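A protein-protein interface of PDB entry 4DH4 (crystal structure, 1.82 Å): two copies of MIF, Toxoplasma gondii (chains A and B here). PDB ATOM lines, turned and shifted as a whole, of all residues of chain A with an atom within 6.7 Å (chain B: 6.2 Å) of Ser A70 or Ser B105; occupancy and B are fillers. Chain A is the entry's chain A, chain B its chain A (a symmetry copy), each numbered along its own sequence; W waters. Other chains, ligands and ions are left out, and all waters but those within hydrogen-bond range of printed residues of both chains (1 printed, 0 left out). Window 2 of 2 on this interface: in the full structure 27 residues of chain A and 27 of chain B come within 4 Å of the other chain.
Water W1 bridges the side-chain hydroxyl of Ser B105 (2.7 Å) and the side-chain amide nitrogen of Asn A73 (3.3 Å).
ND2 of Asn A73 sits at hydrogen-bond distance from O of Ser B105 (3.0 Å).
N of Phe A99 sits at hydrogen-bond distance from O of Glu B106, at 2.9 Å.
Hydrophobic or aromatic side chains of chain A that line the printed part of chain B: Phe A99.
Of the 8 printed residues of chain B, 3 touch a printed residue of chain A.
Printed residues of chain B that touch a printed residue of chain A: Ser B105, Glu B106 and Thr B113.
Among the printed residues, no Asp or Glu carboxylate lies within 4 Å of a Lys or Arg side-chain nitrogen of the other chain.
Among the printed residues, merely in contact across the chains: Ser A70 with Ser B105 (3.8 Å), Ser A70 with Thr B113 (3.8 Å) and Asn A73 with Glu B106 (3.9 Å).
No position is printed for both chains.
Of the 5 pairs that touch across the chains among the printed residues, none has its exchanged pair printed and touching as well.
The backbone carbonyl oxygen of Thr A69 sits close to the side-chain amide oxygen of Asn A73, at 3.0 Å.
OE1 of Glu B106 is in hydrogen-bond range of N of Ser B103 (3.0 Å).
Of chain B, only Ser B105 and Thr B113 come within 4 Å of Ser A70.
Ser B105 touches just these residues of chain A: Ser A70 and Asn A73.
Printed residues of chain B within 4 Å of Asn A73: Ser B105 (3.0 Å) and Glu B106 (3.9 Å).
Printed residues of chain A within 4 Å of Thr B113: Ser A70 (3.8 Å).
Printed residues of chain A within 4 Å of Glu B106: Asn A73 (3.9 Å) and Phe A99 (2.9 Å).
The nearest residue of chain A that does not touch Ser B105 is Phe A99 (4.8 Å).
The nearest printed residue of chain B that does not touch Phe A99 is Ala B108 (4.3 Å).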
ATOM      1  N   GLY A  67     -27.029  38.459   8.537  1.00  0.00           N
ATOM      2  CA  GLY A  67     -26.369  38.340   7.241  1.00  0.00           C
ATOM      3  C   GLY A  67     -25.684  37.002   7.074  1.00  0.00           C
ATOM      4  O   GLY A  67     -25.145  36.712   6.017  1.00  0.00           O
ATOM      5  N   ILE A  68     -25.712  36.180   8.119  1.00  0.00           N
ATOM      6  CA  ILE A  68     -25.079  34.860   8.065  1.00  0.00           C
ATOM      7  C   ILE A  68     -26.069  33.867   7.456  1.00  0.00           C
ATOM      8  O   ILE A  68     -27.069  33.528   8.080  1.00  0.00           O
ATOM      9  CB  ILE A  68     -24.578  34.400   9.474  1.00  0.00           C
ATOM     10  CG1 ILE A  68     -23.563  35.407  10.050  1.00  0.00           C
ATOM     11  CG2 ILE A  68     -23.992  32.965   9.432  1.00  0.00           C
ATOM     12  CD1 ILE A  68     -22.324  35.674   9.154  1.00  0.00           C
ATOM     13  N   THR A  69     -25.812  33.438   6.217  1.00  0.00           N
ATOM     14  CA  THR A  69     -26.717  32.511   5.517  1.00  0.00           C
ATOM     15  C   THR A  69     -25.880  31.585   4.648  1.00  0.00           C
ATOM     16  O   THR A  69     -24.758  31.928   4.308  1.00  0.00           O
ATOM     17  CB  THR A  69     -27.714  33.239   4.578  1.00  0.00           C
ATOM     18  OG1 THR A  69     -27.011  33.773   3.444  1.00  0.00           O
ATOM     19  CG2 THR A  69     -28.457  34.358   5.301  1.00  0.00           C
ATOM     20  N   SER A  70     -26.434  30.446   4.243  1.00  0.00           N
ATOM     21  CA  SER A  70     -25.670  29.527   3.399  1.00  0.00           C
ATOM     22  C   SER A  70     -25.059  30.213   2.160  1.00  0.00           C
ATOM     23  O   SER A  70     -23.872  30.036   1.888  1.00  0.00           O
ATOM     24  CB  SER A  70     -26.507  28.304   2.999  1.00  0.00           C
ATOM     25  OG  SER A  70     -25.659  27.293   2.478  1.00  0.00           O
ATOM     26  N   SER A  71     -25.862  30.994   1.435  1.00  0.00           N
ATOM     27  CA  SER A  71     -25.385  31.631   0.198  1.00  0.00           C
ATOM     28  C   SER A  71     -24.313  32.680   0.477  1.00  0.00           C
ATOM     29  O   SER A  71     -23.279  32.719  -0.197  1.00  0.00           O
ATOM     30  CB  SER A  71     -26.538  32.253  -0.596  1.00  0.00           C
ATOM     31  OG  SER A  71     -27.625  31.356  -0.727  1.00  0.00           O
ATOM     32  N   THR A  72     -24.565  33.529   1.468  1.00  0.00           N
ATOM     33  CA  THR A  72     -23.640  34.611   1.800  1.00  0.00           C
ATOM     34  C   THR A  72     -22.335  34.075   2.394  1.00  0.00           C
ATOM     35  O   THR A  72     -21.253  34.577   2.069  1.00  0.00           O
ATOM     36  CB  THR A  72     -24.320  35.653   2.704  1.00  0.00           C
ATOM     37  OG1 THR A  72     -25.487  36.148   2.029  1.00  0.00           O
ATOM     38  CG2 THR A  72     -23.383  36.810   3.011  1.00  0.00           C
ATOM     39  N   ASN A  73     -22.436  33.052   3.244  1.00  0.00           N
ATOM     40  CA  ASN A  73     -21.249  32.404   3.810  1.00  0.00           C
ATOM     41  C   ASN A  73     -20.371  31.805   2.719  1.00  0.00           C
ATOM     42  O   ASN A  73     -19.143  31.956   2.748  1.00  0.00           O
ATOM     43  CB  ASN A  73     -21.637  31.316   4.822  1.00  0.00           C
ATOM     44  CG  ASN A  73     -22.458  31.855   5.989  1.00  0.00           C
ATOM     45  OD1 ASN A  73     -22.640  33.068   6.141  1.00  0.00           O
ATOM     46  ND2 ASN A  73     -22.970  30.948   6.808  1.00  0.00           N
ATOM     47  N   CYS A  74     -21.002  31.140   1.758  1.00  0.00           N
ATOM     48  CA  CYS A  74     -20.284  30.564   0.627  1.00  0.00           C
ATOM     49  C   CYS A  74     -19.553  31.624  -0.204  1.00  0.00           C
ATOM     50  O   CYS A  74     -18.410  31.415  -0.611  1.00  0.00           O
ATOM     51  CB  CYS A  74     -21.233  29.755  -0.251  1.00  0.00           C
ATOM     52  SG  CYS A  74     -20.369  28.628  -1.340  1.00  0.00           S
ATOM     53  N   LYS A  75     -20.218  32.754  -0.449  1.00  0.00           N
ATOM     54  CA  LYS A  75     -19.612  33.875  -1.164  1.00  0.00           C
ATOM     55  C   LYS A  75     -18.373  34.409  -0.449  1.00  0.00           C
ATOM     56  O   LYS A  75     -17.325  34.600  -1.078  1.00  0.00           O
ATOM     57  CB  LYS A  75     -20.638  34.991  -1.358  1.00  0.00           C
ATOM     58  CG  LYS A  75     -20.133  36.146  -2.196  1.00  0.00           C
ATOM     59  CD  LYS A  75     -21.267  36.777  -2.992  1.00  0.00           C
ATOM     60  CE  LYS A  75     -21.854  37.947  -2.251  1.00  0.00           C
ATOM     61  NZ  LYS A  75     -22.098  39.122  -3.208  1.00  0.00           N
ATOM     62  N   PHE A  99     -18.530  30.630  10.433  1.00  0.00           N
ATOM     63  CA  PHE A  99     -19.374  31.814  10.504  1.00  0.00           C
ATOM     64  C   PHE A  99     -20.205  31.813  11.772  1.00  0.00           C
ATOM     65  O   PHE A  99     -20.695  30.762  12.208  1.00  0.00           O
ATOM     66  CB  PHE A  99     -20.265  31.888   9.263  1.00  0.00           C
ATOM     67  CG  PHE A  99     -19.487  32.007   7.980  1.00  0.00           C
ATOM     68  CD1 PHE A  99     -19.269  33.259   7.397  1.00  0.00           C
ATOM     69  CD2 PHE A  99     -18.941  30.879   7.371  1.00  0.00           C
ATOM     70  CE1 PHE A  99     -18.524  33.380   6.225  1.00  0.00           C
ATOM     71  CE2 PHE A  99     -18.181  30.997   6.187  1.00  0.00           C
ATOM     72  CZ  PHE A  99     -17.983  32.244   5.625  1.00  0.00           C
ATOM     73  N   SER B 103     -23.664  24.759  12.629  1.00  0.00           N
ATOM     74  CA  SER B 103     -24.520  24.255  11.563  1.00  0.00           C
ATOM     75  C   SER B 103     -23.659  23.996  10.321  1.00  0.00           C
ATOM     76  O   SER B 103     -22.632  24.657  10.143  1.00  0.00           O
ATOM     77  CB  SER B 103     -25.620  25.270  11.243  1.00  0.00           C
ATOM     78  OG  SER B 103     -26.431  25.516  12.380  1.00  0.00           O
ATOM     79  N   PRO B 104     -24.059  23.032   9.468  1.00  0.00           N
ATOM     80  CA  PRO B 104     -23.282  22.789   8.240  1.00  0.00           C
ATOM     81  C   PRO B 104     -23.101  24.045   7.373  1.00  0.00           C
ATOM     82  O   PRO B 104     -22.019  24.258   6.832  1.00  0.00           O
ATOM     83  CB  PRO B 104     -24.111  21.732   7.498  1.00  0.00           C
ATOM     84  CG  PRO B 104     -24.875  21.038   8.562  1.00  0.00           C
ATOM     85  CD  PRO B 104     -25.212  22.111   9.563  1.00  0.00           C
ATOM     86  N   SER B 105     -24.135  24.880   7.263  1.00  0.00           N
ATOM     87  CA  SER B 105     -24.043  26.105   6.452  1.00  0.00           C
ATOM     88  C   SER B 105     -23.054  27.141   7.013  1.00  0.00           C
ATOM     89  O   SER B 105     -22.651  28.055   6.296  1.00  0.00           O
ATOM     90  CB  SER B 105     -25.418  26.758   6.300  1.00  0.00           C
ATOM     91  OG  SER B 105     -25.864  27.220   7.565  1.00  0.00           O
ATOM     92  N   GLU B 106     -22.672  26.989   8.282  1.00  0.00           N
ATOM     93  CA  GLU B 106     -21.741  27.915   8.949  1.00  0.00           C
ATOM     94  C   GLU B 106     -20.280  27.502   8.799  1.00  0.00           C
ATOM     95  O   GLU B 106     -19.401  28.109   9.397  1.00  0.00           O
ATOM     96  CB  GLU B 106     -22.059  28.016  10.450  1.00  0.00           C
ATOM     97  CG  GLU B 106     -23.342  28.762  10.764  1.00  0.00           C
ATOM     98  CD  GLU B 106     -23.794  28.603  12.204  1.00  0.00           C
ATOM     99  OE1 GLU B 106     -23.307  27.695  12.915  1.00  0.00           O
ATOM    100  OE2 GLU B 106     -24.660  29.399  12.627  1.00  0.00           O
ATOM    101  N   TRP B 107     -20.018  26.468   8.008  1.00  0.00           N
ATOM    102  CA  TRP B 107     -18.670  25.925   7.908  1.00  0.00           C
ATOM    103  C   TRP B 107     -18.313  25.720   6.443  1.00  0.00           C
ATOM    104  O   TRP B 107     -19.040  25.041   5.709  1.00  0.00           O
ATOM    105  CB  TRP B 107     -18.587  24.599   8.672  1.00  0.00           C
ATOM    106  CG  TRP B 107     -17.192  24.185   9.089  1.00  0.00           C
ATOM    107  CD1 TRP B 107     -16.091  24.051   8.286  1.00  0.00           C
ATOM    108  CD2 TRP B 107     -16.773  23.809  10.407  1.00  0.00           C
ATOM    109  NE1 TRP B 107     -15.008  23.639   9.034  1.00  0.00           N
ATOM    110  CE2 TRP B 107     -15.401  23.481  10.336  1.00  0.00           C
ATOM    111  CE3 TRP B 107     -17.421  23.741  11.648  1.00  0.00           C
ATOM    112  CZ2 TRP B 107     -14.663  23.077  11.463  1.00  0.00           C
ATOM    113  CZ3 TRP B 107     -16.691  23.337  12.766  1.00  0.00           C
ATOM    114  CH2 TRP B 107     -15.327  23.009  12.664  1.00  0.00           C
ATOM    115  N   ALA B 108     -17.209  26.336   6.019  1.00  0.00           N
ATOM    116  CA  ALA B 108     -16.725  26.217   4.647  1.00  0.00           C
ATOM    117  C   ALA B 108     -15.324  25.614   4.584  1.00  0.00           C
ATOM    118  O   ALA B 108     -14.507  25.812   5.476  1.00  0.00           O
ATOM    119  CB  ALA B 108     -16.730  27.581   3.969  1.00  0.00           C
ATOM    120  N   THR B 113     -19.458  25.480   1.255  1.00  0.00           N
ATOM    121  CA  THR B 113     -19.972  25.157   2.596  1.00  0.00           C
ATOM    122  C   THR B 113     -20.353  23.685   2.701  1.00  0.00           C
ATOM    123  O   THR B 113     -20.595  23.014   1.690  1.00  0.00           O
ATOM    124  CB  THR B 113     -21.211  25.989   3.007  1.00  0.00           C
ATOM    125  OG1 THR B 113     -22.177  25.972   1.950  1.00  0.00           O
ATOM    126  CG2 THR B 113     -20.834  27.432   3.353  1.00  0.00           C
ATOM    127  N   PHE B 114     -20.424  23.191   3.934  1.00  0.00           N
ATOM    128  CA  PHE B 114     -20.829  21.816   4.195  1.00  0.00           C
ATOM    129  C   PHE B 114     -22.341  21.629   4.116  1.00  0.00           C
ATOM    130  O   PHE B 114     -23.116  22.583   4.003  1.00  0.00           O
ATOM    131  CB  PHE B 114     -20.305  21.352   5.557  1.00  0.00           C
ATOM    132  CG  PHE B 114     -18.858  20.974   5.545  1.00  0.00           C
ATOM    133  CD1 PHE B 114     -17.882  21.898   5.903  1.00  0.00           C
ATOM    134  CD2 PHE B 114     -18.466  19.694   5.169  1.00  0.00           C
ATOM    135  CE1 PHE B 114     -16.534  21.551   5.891  1.00  0.00           C
ATOM    136  CE2 PHE B 114     -17.126  19.339   5.145  1.00  0.00           C
ATOM    137  CZ  PHE B 114     -16.155  20.268   5.512  1.00  0.00           C
ATOM    138  OXT PHE B 114     -22.822  20.496   4.167  1.00  0.00           O
HETATM  139  O   HOH W   1     -25.822  29.917   8.014  1.00  0.00           O
